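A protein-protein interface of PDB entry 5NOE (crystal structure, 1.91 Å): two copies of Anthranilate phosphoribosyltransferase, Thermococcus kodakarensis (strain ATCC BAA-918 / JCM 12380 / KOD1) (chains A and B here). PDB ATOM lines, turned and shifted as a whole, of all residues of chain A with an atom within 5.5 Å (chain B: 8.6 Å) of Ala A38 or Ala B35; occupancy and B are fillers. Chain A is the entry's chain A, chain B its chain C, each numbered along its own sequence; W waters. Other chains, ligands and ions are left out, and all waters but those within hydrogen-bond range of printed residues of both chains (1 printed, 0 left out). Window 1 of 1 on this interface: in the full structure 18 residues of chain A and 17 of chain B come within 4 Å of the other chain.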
ATOM      1  N   VAL A  31      37.771  -3.814  26.854  1.00  0.00           N
ATOM      2  CA  VAL A  31      36.679  -4.565  26.224  1.00  0.00           C
ATOM      3  C   VAL A  31      36.088  -5.572  27.204  1.00  0.00           C
ATOM      4  O   VAL A  31      34.861  -5.741  27.290  1.00  0.00           O
ATOM      5  CB  VAL A  31      37.151  -5.273  24.940  1.00  0.00           C
ATOM      6  CG1 VAL A  31      36.012  -6.154  24.378  1.00  0.00           C
ATOM      7  CG2 VAL A  31      37.605  -4.278  23.887  1.00  0.00           C
ATOM      8  N   ILE A  33      36.506  -5.497  30.578  1.00  0.00           N
ATOM      9  CA  ILE A  33      35.925  -4.741  31.686  1.00  0.00           C
ATOM     10  C   ILE A  33      34.512  -4.287  31.331  1.00  0.00           C
ATOM     11  O   ILE A  33      33.571  -4.467  32.109  1.00  0.00           O
ATOM     12  CB  ILE A  33      36.800  -3.528  32.050  1.00  0.00           C
ATOM     13  CG1 ILE A  33      38.195  -3.946  32.510  1.00  0.00           C
ATOM     14  CG2 ILE A  33      36.096  -2.728  33.137  1.00  0.00           C
ATOM     15  CD1 ILE A  33      39.137  -2.727  32.670  1.00  0.00           C
ATOM     16  N   GLY A  34      34.357  -3.662  30.160  1.00  0.00           N
ATOM     17  CA  GLY A  34      33.043  -3.210  29.723  1.00  0.00           C
ATOM     18  C   GLY A  34      32.014  -4.331  29.665  1.00  0.00           C
ATOM     19  O   GLY A  34      30.873  -4.159  30.099  1.00  0.00           O
ATOM     20  N   ALA A  35      32.393  -5.491  29.111  1.00  0.00           N
ATOM     21  CA  ALA A  35      31.463  -6.625  29.059  1.00  0.00           C
ATOM     22  C   ALA A  35      31.083  -7.087  30.466  1.00  0.00           C
ATOM     23  O   ALA A  35      29.900  -7.282  30.780  1.00  0.00           O
ATOM     24  CB  ALA A  35      32.082  -7.778  28.265  1.00  0.00           C
ATOM     25  N   TYR A  36      32.077  -7.229  31.343  1.00  0.00           N
ATOM     26  CA  TYR A  36      31.799  -7.715  32.690  1.00  0.00           C
ATOM     27  C   TYR A  36      30.851  -6.771  33.428  1.00  0.00           C
ATOM     28  O   TYR A  36      29.882  -7.217  34.058  1.00  0.00           O
ATOM     29  CB  TYR A  36      33.095  -7.875  33.466  1.00  0.00           C
ATOM     30  CG  TYR A  36      33.696  -9.283  33.443  1.00  0.00           C
ATOM     31  CD1 TYR A  36      32.944 -10.395  33.818  1.00  0.00           C
ATOM     32  CD2 TYR A  36      35.003  -9.487  33.031  1.00  0.00           C
ATOM     33  CE1 TYR A  36      33.497 -11.672  33.804  1.00  0.00           C
ATOM     34  CE2 TYR A  36      35.565 -10.768  33.013  1.00  0.00           C
ATOM     35  CZ  TYR A  36      34.804 -11.855  33.390  1.00  0.00           C
ATOM     36  OH  TYR A  36      35.353 -13.129  33.374  1.00  0.00           O
ATOM     37  N   LEU A  37      31.120  -5.461  33.377  1.00  0.00           N
ATOM     38  CA  LEU A  37      30.302  -4.548  34.173  1.00  0.00           C
ATOM     39  C   LEU A  37      28.869  -4.491  33.655  1.00  0.00           C
ATOM     40  O   LEU A  37      27.921  -4.500  34.455  1.00  0.00           O
ATOM     41  CB  LEU A  37      30.927  -3.155  34.203  1.00  0.00           C
ATOM     42  CG  LEU A  37      32.246  -3.037  34.998  1.00  0.00           C
ATOM     43  CD1 LEU A  37      32.734  -1.615  34.882  1.00  0.00           C
ATOM     44  CD2 LEU A  37      32.079  -3.455  36.472  1.00  0.00           C
ATOM     45  N   ALA A  38      28.686  -4.427  32.329  1.00  0.00           N
ATOM     46  CA  ALA A  38      27.338  -4.395  31.755  1.00  0.00           C
ATOM     47  C   ALA A  38      26.587  -5.705  31.974  1.00  0.00           C
ATOM     48  O   ALA A  38      25.375  -5.698  32.245  1.00  0.00           O
ATOM     49  CB  ALA A  38      27.404  -4.069  30.265  1.00  0.00           C
ATOM     50  N   ALA A  39      27.276  -6.845  31.862  1.00  0.00           N
ATOM     51  CA  ALA A  39      26.573  -8.112  32.027  1.00  0.00           C
ATOM     52  C   ALA A  39      26.145  -8.302  33.473  1.00  0.00           C
ATOM     53  O   ALA A  39      25.021  -8.735  33.746  1.00  0.00           O
ATOM     54  CB  ALA A  39      27.451  -9.276  31.573  1.00  0.00           C
ATOM     55  N   LEU A  40      27.023  -7.970  34.409  1.00  0.00           N
ATOM     56  CA  LEU A  40      26.670  -8.118  35.815  1.00  0.00           C
ATOM     57  C   LEU A  40      25.533  -7.181  36.198  1.00  0.00           C
ATOM     58  O   LEU A  40      24.680  -7.541  37.015  1.00  0.00           O
ATOM     59  CB  LEU A  40      27.887  -7.854  36.679  1.00  0.00           C
ATOM     60  CG  LEU A  40      27.651  -7.990  38.176  1.00  0.00           C
ATOM     61  CD1 LEU A  40      27.279  -9.404  38.510  1.00  0.00           C
ATOM     62  CD2 LEU A  40      28.897  -7.528  38.955  1.00  0.00           C
ATOM     63  N   GLN A  41      25.501  -5.992  35.608  1.00  0.00           N
ATOM     64  CA  GLN A  41      24.414  -5.067  35.889  1.00  0.00           C
ATOM     65  C   GLN A  41      23.105  -5.586  35.294  1.00  0.00           C
ATOM     66  O   GLN A  41      22.035  -5.483  35.922  1.00  0.00           O
ATOM     67  CB  GLN A  41      24.761  -3.685  35.338  1.00  0.00           C
ATOM     68  CG  GLN A  41      23.924  -2.541  35.882  1.00  0.00           C
ATOM     69  CD  GLN A  41      24.181  -2.245  37.360  1.00  0.00           C
ATOM     70  OE1 GLN A  41      25.172  -2.683  37.928  1.00  0.00           O
ATOM     71  NE2 GLN A  41      23.288  -1.471  37.975  1.00  0.00           N
ATOM     72  N   THR A  42      23.171  -6.151  34.085  1.00  0.00           N
ATOM     73  CA  THR A  42      21.978  -6.735  33.488  1.00  0.00           C
ATOM     74  C   THR A  42      21.449  -7.873  34.336  1.00  0.00           C
ATOM     75  O   THR A  42      20.239  -7.972  34.563  1.00  0.00           O
ATOM     76  CB  THR A  42      22.282  -7.212  32.070  1.00  0.00           C
ATOM     77  OG1 THR A  42      22.843  -6.125  31.321  1.00  0.00           O
ATOM     78  CG2 THR A  42      21.015  -7.701  31.369  1.00  0.00           C
ATOM     79  N   LYS A  43      22.343  -8.747  34.820  1.00  0.00           N
ATOM     80  CA  LYS A  43      21.907  -9.873  35.644  1.00  0.00           C
ATOM     81  C   LYS A  43      21.375  -9.394  36.990  1.00  0.00           C
ATOM     82  O   LYS A  43      20.397  -9.943  37.511  1.00  0.00           O
ATOM     83  CB  LYS A  43      23.064 -10.860  35.859  1.00  0.00           C
ATOM     84  CG  LYS A  43      22.765 -11.977  36.852  1.00  0.00           C
ATOM     85  CD  LYS A  43      23.894 -13.001  36.959  1.00  0.00           C
ATOM     86  CE  LYS A  43      25.064 -12.480  37.804  1.00  0.00           C
ATOM     87  NZ  LYS A  43      24.683 -12.144  39.234  1.00  0.00           N
ATOM     88  N   LEU A 162      30.826   3.839  29.498  1.00  0.00           N
ATOM     89  CA  LEU A 162      29.587   3.056  29.475  1.00  0.00           C
ATOM     90  C   LEU A 162      28.383   3.923  29.803  1.00  0.00           C
ATOM     91  O   LEU A 162      27.316   3.750  29.202  1.00  0.00           O
ATOM     92  CB  LEU A 162      29.660   1.869  30.442  1.00  0.00           C
ATOM     93  CG  LEU A 162      30.640   0.728  30.131  1.00  0.00           C
ATOM     94  CD1 LEU A 162      30.344  -0.506  30.976  1.00  0.00           C
ATOM     95  CD2 LEU A 162      30.668   0.388  28.651  1.00  0.00           C
ATOM     96  N   ILE A 164      26.361   3.924  32.191  1.00  0.00           N
ATOM     97  CA  ILE A 164      25.306   3.249  32.927  1.00  0.00           C
ATOM     98  C   ILE A 164      25.770   3.124  34.368  1.00  0.00           C
ATOM     99  O   ILE A 164      26.965   3.185  34.674  1.00  0.00           O
ATOM    100  CB  ILE A 164      24.974   1.847  32.361  1.00  0.00           C
ATOM    101  CG1 ILE A 164      26.237   0.975  32.358  1.00  0.00           C
ATOM    102  CG2 ILE A 164      24.373   1.950  30.975  1.00  0.00           C
ATOM    103  CD1 ILE A 164      25.985  -0.537  32.351  1.00  0.00           C
ATOM    104  N   MET B   1      24.651   4.001  24.754  1.00  0.00           N
ATOM    105  CA  MET B   1      24.497   4.215  26.190  1.00  0.00           C
ATOM    106  C   MET B   1      23.014   4.281  26.571  1.00  0.00           C
ATOM    107  O   MET B   1      22.588   3.711  27.579  1.00  0.00           O
ATOM    108  CB  MET B   1      25.198   5.506  26.621  1.00  0.00           C
ATOM    109  CG  MET B   1      26.531   5.738  26.025  1.00  0.00           C
ATOM    110  SD  MET B   1      27.066   7.441  26.203  1.00  0.00           S
ATOM    111  CE  MET B   1      26.240   7.899  27.637  1.00  0.00           C
ATOM    112  N   LEU B   4      22.031   0.954  25.572  1.00  0.00           N
ATOM    113  CA  LEU B   4      22.651   0.104  26.587  1.00  0.00           C
ATOM    114  C   LEU B   4      21.894   0.170  27.905  1.00  0.00           C
ATOM    115  O   LEU B   4      21.661  -0.862  28.541  1.00  0.00           O
ATOM    116  CB  LEU B   4      24.115   0.483  26.802  1.00  0.00           C
ATOM    117  CG  LEU B   4      24.869  -0.356  27.824  1.00  0.00           C
ATOM    118  CD1 LEU B   4      24.965  -1.861  27.398  1.00  0.00           C
ATOM    119  CD2 LEU B   4      26.256   0.234  28.093  1.00  0.00           C
ATOM    120  N   ALA B   5      21.470   1.367  28.321  1.00  0.00           N
ATOM    121  CA  ALA B   5      20.731   1.479  29.577  1.00  0.00           C
ATOM    122  C   ALA B   5      19.414   0.710  29.498  1.00  0.00           C
ATOM    123  O   ALA B   5      19.032   0.007  30.441  1.00  0.00           O
ATOM    124  CB  ALA B   5      20.501   2.961  29.920  1.00  0.00           C
ATOM    125  N   ILE B   7      18.689  -1.956  27.560  1.00  0.00           N
ATOM    126  CA  ILE B   7      19.007  -3.383  27.624  1.00  0.00           C
ATOM    127  C   ILE B   7      19.378  -3.782  29.042  1.00  0.00           C
ATOM    128  O   ILE B   7      18.903  -4.793  29.567  1.00  0.00           O
ATOM    129  CB  ILE B   7      20.141  -3.720  26.635  1.00  0.00           C
ATOM    130  CG1 ILE B   7      19.672  -3.589  25.182  1.00  0.00           C
ATOM    131  CG2 ILE B   7      20.774  -5.101  26.952  1.00  0.00           C
ATOM    132  CD1 ILE B   7      20.860  -3.436  24.203  1.00  0.00           C
ATOM    133  N   VAL B   8      20.274  -3.017  29.670  1.00  0.00           N
ATOM    134  CA  VAL B   8      20.711  -3.339  31.028  1.00  0.00           C
ATOM    135  C   VAL B   8      19.533  -3.297  32.002  1.00  0.00           C
ATOM    136  O   VAL B   8      19.504  -4.021  33.010  1.00  0.00           O
ATOM    137  CB  VAL B   8      21.851  -2.371  31.414  1.00  0.00           C
ATOM    138  CG1 VAL B   8      21.925  -2.148  32.904  1.00  0.00           C
ATOM    139  CG2 VAL B   8      23.200  -2.884  30.845  1.00  0.00           C
ATOM    140  N   ASP B   9      18.540  -2.480  31.705  1.00  0.00           N
ATOM    141  CA  ASP B   9      17.335  -2.429  32.516  1.00  0.00           C
ATOM    142  C   ASP B   9      16.401  -3.614  32.263  1.00  0.00           C
ATOM    143  O   ASP B   9      15.407  -3.760  32.983  1.00  0.00           O
ATOM    144  CB  ASP B   9      16.621  -1.110  32.242  1.00  0.00           C
ATOM    145  CG  ASP B   9      15.461  -0.865  33.188  1.00  0.00           C
ATOM    146  OD1 ASP B   9      15.563  -1.243  34.377  1.00  0.00           O
ATOM    147  OD2 ASP B   9      14.446  -0.304  32.732  1.00  0.00           O
ATOM    148  N   LEU B  21      20.689  -0.085  16.635  1.00  0.00           N
ATOM    149  CA  LEU B  21      21.781  -0.587  17.468  1.00  0.00           C
ATOM    150  C   LEU B  21      22.910  -1.146  16.608  1.00  0.00           C
ATOM    151  O   LEU B  21      24.089  -0.884  16.878  1.00  0.00           O
ATOM    152  CB  LEU B  21      21.284  -1.633  18.447  1.00  0.00           C
ATOM    153  CG  LEU B  21      22.440  -2.249  19.241  1.00  0.00           C
ATOM    154  CD1 LEU B  21      23.172  -1.180  20.014  1.00  0.00           C
ATOM    155  CD2 LEU B  21      21.936  -3.299  20.171  1.00  0.00           C
ATOM    156  N   LEU B  25      26.732   0.022  16.989  1.00  0.00           N
ATOM    157  CA  LEU B  25      27.830  -0.917  17.230  1.00  0.00           C
ATOM    158  C   LEU B  25      28.895  -0.789  16.157  1.00  0.00           C
ATOM    159  O   LEU B  25      30.099  -0.826  16.436  1.00  0.00           O
ATOM    160  CB  LEU B  25      27.292  -2.355  17.233  1.00  0.00           C
ATOM    161  CG  LEU B  25      26.378  -2.819  18.371  1.00  0.00           C
ATOM    162  CD1 LEU B  25      25.792  -4.198  18.061  1.00  0.00           C
ATOM    163  CD2 LEU B  25      27.190  -2.859  19.661  1.00  0.00           C
ATOM    164  N   ASP B  29      33.565   2.167  19.860  1.00  0.00           N
ATOM    165  CA  ASP B  29      34.796   1.627  20.418  1.00  0.00           C
ATOM    166  C   ASP B  29      34.561   0.224  20.958  1.00  0.00           C
ATOM    167  O   ASP B  29      33.449  -0.138  21.343  1.00  0.00           O
ATOM    168  CB  ASP B  29      35.328   2.497  21.562  1.00  0.00           C
ATOM    169  CG  ASP B  29      36.610   1.909  22.164  1.00  0.00           C
ATOM    170  OD1 ASP B  29      37.501   1.540  21.352  1.00  0.00           O
ATOM    171  OD2 ASP B  29      36.709   1.734  23.410  1.00  0.00           O
ATOM    172  N   GLY B  30      35.645  -0.552  21.033  1.00  0.00           N
ATOM    173  CA  GLY B  30      35.553  -1.908  21.540  1.00  0.00           C
ATOM    174  C   GLY B  30      34.942  -2.003  22.923  1.00  0.00           C
ATOM    175  O   GLY B  30      34.223  -2.958  23.224  1.00  0.00           O
ATOM    176  N   VAL B  31      35.221  -1.024  23.789  1.00  0.00           N
ATOM    177  CA  VAL B  31      34.632  -1.075  25.131  1.00  0.00           C
ATOM    178  C   VAL B  31      33.104  -1.121  25.045  1.00  0.00           C
ATOM    179  O   VAL B  31      32.439  -1.910  25.744  1.00  0.00           O
ATOM    180  CB  VAL B  31      35.116   0.118  25.976  1.00  0.00           C
ATOM    181  CG1 VAL B  31      34.398   0.141  27.346  1.00  0.00           C
ATOM    182  CG2 VAL B  31      36.623   0.046  26.175  1.00  0.00           C
ATOM    183  N   LEU B  32      32.520  -0.279  24.187  1.00  0.00           N
ATOM    184  CA  LEU B  32      31.065  -0.236  24.091  1.00  0.00           C
ATOM    185  C   LEU B  32      30.517  -1.484  23.424  1.00  0.00           C
ATOM    186  O   LEU B  32      29.448  -1.974  23.811  1.00  0.00           O
ATOM    187  CB  LEU B  32      30.602   0.986  23.319  1.00  0.00           C
ATOM    188  CG  LEU B  32      30.263   2.116  24.262  1.00  0.00           C
ATOM    189  CD1 LEU B  32      31.555   2.852  24.574  1.00  0.00           C
ATOM    190  CD2 LEU B  32      29.232   3.022  23.613  1.00  0.00           C
ATOM    191  N   ILE B  33      31.211  -1.989  22.400  1.00  0.00           N
ATOM    192  CA  ILE B  33      30.751  -3.218  21.746  1.00  0.00           C
ATOM    193  C   ILE B  33      30.727  -4.368  22.738  1.00  0.00           C
ATOM    194  O   ILE B  33      29.754  -5.142  22.807  1.00  0.00           O
ATOM    195  CB  ILE B  33      31.631  -3.553  20.532  1.00  0.00           C
ATOM    196  CG1 ILE B  33      31.622  -2.411  19.540  1.00  0.00           C
ATOM    197  CG2 ILE B  33      31.145  -4.886  19.898  1.00  0.00           C
ATOM    198  CD1 ILE B  33      32.563  -2.610  18.329  1.00  0.00           C
ATOM    199  N   GLY B  34      31.814  -4.512  23.499  1.00  0.00           N
ATOM    200  CA  GLY B  34      31.865  -5.542  24.521  1.00  0.00           C
ATOM    201  C   GLY B  34      30.697  -5.429  25.480  1.00  0.00           C
ATOM    202  O   GLY B  34      29.994  -6.409  25.743  1.00  0.00           O
ATOM    203  N   ALA B  35      30.420  -4.209  25.952  1.00  0.00           N
ATOM    204  CA  ALA B  35      29.317  -4.011  26.892  1.00  0.00           C
ATOM    205  C   ALA B  35      27.972  -4.398  26.269  1.00  0.00           C
ATOM    206  O   ALA B  35      27.192  -5.136  26.878  1.00  0.00           O
ATOM    207  CB  ALA B  35      29.300  -2.558  27.377  1.00  0.00           C
ATOM    208  N   TYR B  36      27.695  -3.917  25.055  1.00  0.00           N
ATOM    209  CA  TYR B  36      26.422  -4.225  24.393  1.00  0.00           C
ATOM    210  C   TYR B  36      26.259  -5.719  24.188  1.00  0.00           C
ATOM    211  O   TYR B  36      25.192  -6.283  24.473  1.00  0.00           O
ATOM    212  CB  TYR B  36      26.323  -3.533  23.038  1.00  0.00           C
ATOM    213  CG  TYR B  36      25.719  -2.160  23.069  1.00  0.00           C
ATOM    214  CD1 TYR B  36      24.375  -1.982  23.411  1.00  0.00           C
ATOM    215  CD2 TYR B  36      26.478  -1.044  22.764  1.00  0.00           C
ATOM    216  CE1 TYR B  36      23.821  -0.728  23.438  1.00  0.00           C
ATOM    217  CE2 TYR B  36      25.928   0.232  22.793  1.00  0.00           C
ATOM    218  CZ  TYR B  36      24.590   0.381  23.136  1.00  0.00           C
ATOM    219  OH  TYR B  36      24.021   1.636  23.172  1.00  0.00           O
ATOM    220  N   LEU B  37      27.315  -6.389  23.712  1.00  0.00           N
ATOM    221  CA  LEU B  37      27.163  -7.809  23.393  1.00  0.00           C
ATOM    222  C   LEU B  37      26.979  -8.643  24.659  1.00  0.00           C
ATOM    223  O   LEU B  37      26.164  -9.581  24.679  1.00  0.00           O
ATOM    224  CB  LEU B  37      28.361  -8.296  22.568  1.00  0.00           C
ATOM    225  CG  LEU B  37      28.461  -7.716  21.155  1.00  0.00           C
ATOM    226  CD1 LEU B  37      29.665  -8.330  20.417  1.00  0.00           C
ATOM    227  CD2 LEU B  37      27.161  -7.948  20.395  1.00  0.00           C
ATOM    228  N   ALA B  38      27.701  -8.312  25.736  1.00  0.00           N
ATOM    229  CA  ALA B  38      27.532  -9.085  26.969  1.00  0.00           C
ATOM    230  C   ALA B  38      26.168  -8.818  27.627  1.00  0.00           C
ATOM    231  O   ALA B  38      25.490  -9.756  28.083  1.00  0.00           O
ATOM    232  CB  ALA B  38      28.690  -8.790  27.937  1.00  0.00           C
ATOM    233  N   ALA B  39      25.737  -7.555  27.662  1.00  0.00           N
ATOM    234  CA  ALA B  39      24.435  -7.219  28.245  1.00  0.00           C
ATOM    235  C   ALA B  39      23.294  -7.849  27.461  1.00  0.00           C
ATOM    236  O   ALA B  39      22.390  -8.454  28.038  1.00  0.00           O
ATOM    237  CB  ALA B  39      24.256  -5.700  28.291  1.00  0.00           C
ATOM    238  N   LEU B  40      23.297  -7.662  26.141  1.00  0.00           N
ATOM    239  CA  LEU B  40      22.297  -8.268  25.270  1.00  0.00           C
ATOM    240  C   LEU B  40      22.217  -9.782  25.461  1.00  0.00           C
ATOM    241  O   LEU B  40      21.121 -10.351  25.554  1.00  0.00           O
ATOM    242  CB  LEU B  40      22.637  -7.902  23.826  1.00  0.00           C
ATOM    243  CG  LEU B  40      21.531  -7.879  22.792  1.00  0.00           C
ATOM    244  CD1 LEU B  40      20.531  -6.793  23.127  1.00  0.00           C
ATOM    245  CD2 LEU B  40      22.149  -7.647  21.438  1.00  0.00           C
ATOM    246  N   GLN B  41      23.371 -10.458  25.554  1.00  0.00           N
ATOM    247  CA  GLN B  41      23.356 -11.904  25.761  1.00  0.00           C
ATOM    248  C   GLN B  41      22.849 -12.269  27.155  1.00  0.00           C
ATOM    249  O   GLN B  41      22.212 -13.318  27.341  1.00  0.00           O
ATOM    250  CB  GLN B  41      24.759 -12.467  25.512  1.00  0.00           C
ATOM    251  CG  GLN B  41      24.856 -13.991  25.523  1.00  0.00           C
ATOM    252  CD  GLN B  41      24.120 -14.653  24.348  1.00  0.00           C
ATOM    253  OE1 GLN B  41      24.015 -14.097  23.236  1.00  0.00           O
ATOM    254  NE2 GLN B  41      23.605 -15.841  24.599  1.00  0.00           N
ATOM    255  N   THR B  42      23.076 -11.413  28.143  1.00  0.00           N
ATOM    256  CA  THR B  42      22.539 -11.704  29.468  1.00  0.00           C
ATOM    257  C   THR B  42      21.016 -11.556  29.488  1.00  0.00           C
ATOM    258  O   THR B  42      20.324 -12.357  30.121  1.00  0.00           O
ATOM    259  CB  THR B  42      23.195 -10.782  30.489  1.00  0.00           C
ATOM    260  OG1 THR B  42      24.615 -10.881  30.347  1.00  0.00           O
ATOM    261  CG2 THR B  42      22.774 -11.119  31.910  1.00  0.00           C
ATOM    262  N   LYS B  43      20.478 -10.564  28.770  1.00  0.00           N
ATOM    263  CA  LYS B  43      19.031 -10.343  28.739  1.00  0.00           C
ATOM    264  C   LYS B  43      18.295 -11.438  27.951  1.00  0.00           C
ATOM    265  O   LYS B  43      17.244 -11.934  28.384  1.00  0.00           O
ATOM    266  CB  LYS B  43      18.734  -8.964  28.148  1.00  0.00           C
ATOM    267  CG  LYS B  43      17.242  -8.660  28.022  1.00  0.00           C
ATOM    268  CD  LYS B  43      16.964  -7.290  27.421  1.00  0.00           C
ATOM    269  CE  LYS B  43      17.224  -7.237  25.907  1.00  0.00           C
ATOM    270  NZ  LYS B  43      16.207  -7.940  25.019  1.00  0.00           N
ATOM    271  N   VAL B 158      36.264  -8.105  19.018  1.00  0.00           N
ATOM    272  CA  VAL B 158      35.527  -8.094  20.278  1.00  0.00           C
ATOM    273  C   VAL B 158      34.903  -9.456  20.537  1.00  0.00           C
ATOM    274  O   VAL B 158      35.051 -10.015  21.630  1.00  0.00           O
ATOM    275  CB  VAL B 158      34.470  -6.973  20.307  1.00  0.00           C
ATOM    276  CG1 VAL B 158      33.676  -7.066  21.617  1.00  0.00           C
ATOM    277  CG2 VAL B 158      35.147  -5.638  20.233  1.00  0.00           C
ATOM    278  N   LEU B 162      35.834 -11.711  23.909  1.00  0.00           N
ATOM    279  CA  LEU B 162      34.834 -12.060  24.916  1.00  0.00           C
ATOM    280  C   LEU B 162      34.704 -13.568  25.067  1.00  0.00           C
ATOM    281  O   LEU B 162      34.474 -14.069  26.176  1.00  0.00           O
ATOM    282  CB  LEU B 162      33.476 -11.449  24.558  1.00  0.00           C
ATOM    283  CG  LEU B 162      33.278  -9.935  24.456  1.00  0.00           C
ATOM    284  CD1 LEU B 162      31.793  -9.631  24.509  1.00  0.00           C
ATOM    285  CD2 LEU B 162      34.011  -9.148  25.521  1.00  0.00           C
ATOM    286  N   ILE B 164      32.356 -15.516  24.643  1.00  0.00           N
ATOM    287  CA  ILE B 164      31.023 -16.036  24.945  1.00  0.00           C
ATOM    288  C   ILE B 164      30.217 -16.042  23.659  1.00  0.00           C
ATOM    289  O   ILE B 164      30.563 -15.379  22.682  1.00  0.00           O
ATOM    290  CB  ILE B 164      30.299 -15.198  26.025  1.00  0.00           C
ATOM    291  CG1 ILE B 164      30.205 -13.744  25.566  1.00  0.00           C
ATOM    292  CG2 ILE B 164      31.029 -15.284  27.361  1.00  0.00           C
ATOM    293  CD1 ILE B 164      29.364 -12.833  26.490  1.00  0.00           C
HETATM  294  O   HOH W   1      18.177  -6.582  33.729  1.00  0.00           O
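The backbone carbonyl oxygen (O) of Ala A38 sits at hydrogen-bond distance from the side-chain hydroxyl (OG1) of Thr A42.
The side-chain hydroxyl (OH) of Tyr B36 is in hydrogen-bond range of the backbone NH (N) of Met B1, 2.9 Å away.
The backbone NH (N) of Leu B4 sits at hydrogen-bond distance from the side-chain hydroxyl (OH) of Tyr B36, at 3.2 Å.
The backbone NH (N) of Val B31 sits at hydrogen-bond distance from the side-chain carboxylate (OD2) of Asp B29, 3.2 Å away.
OG1 of Thr B42 is in hydrogen-bond range of O of Ala B38 (2.7 Å).
Ala B35 touches Gly A34 (CB to O, 3.5 Å).
Ala A35 touches Gly B34 (CB to O, 3.5 Å).
Val B8 touches Ala A38.
Ala A39 touches Ala B38.
CG1 of Val B8 touches CG of Gln A41, at 3.6 Å.
Thr B42 touches Thr A42 (CB to CG2, 3.9 Å).
Thr A42 touches Lys B43.
Thr B42 touches Lys A43 (CG2 to N, 3.8 Å).
Met B1 touches Leu A162.
Val B8 touches Ile A164 (CG2 to CD1, 3.9 Å).
Of chain A, only Gly A34, Ala A35, Ala A38 and Leu A162 come within 4 Å of Ala B35.
Of chain B, only Ala B38 and Thr B42 come within 4 Å of Ala A39.
Printed residues of chain A within 4 Å of Lys B43: Thr A42.
Of the printed residues of chain A, Leu B162 touches Val A31 (3.8 Å) and Ala A35 (3.6 Å).
Of the printed residues of chain A, Thr B42 touches Ala A39 (3.5 Å), Thr A42 (3.9 Å) and Lys A43 (3.8 Å).
Of the 26 printed residues of chain B, 14 touch a printed residue of chain A.
Hydrophobic or aromatic side chains of chain B within 4 Å of the printed part of chain A: Met B1, Leu B4, Val B8, Val B31, Ala B35, Ala B38, Ala B39, Val B158 and Leu B162.
Ala A35 touches Leu B162, and with the chains exchanged Leu A162 touches Ala B35.
Ala A39 touches Ala B38, but with the chains exchanged Ala A38 does not touch Ala B39 (4.1 Å).
Ala A39 touches Thr B42, and with the chains exchanged Thr A42 touches Ala B39.
Thr B42 touches its own counterpart, Thr A42.
Positions printed for both chains: 31, 33, 34, 35, 36, 37, 38, 39, 40, 41, 42, 43, 162 and 164.
Water W1 bridges O of Thr A42 and O of Val B8.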
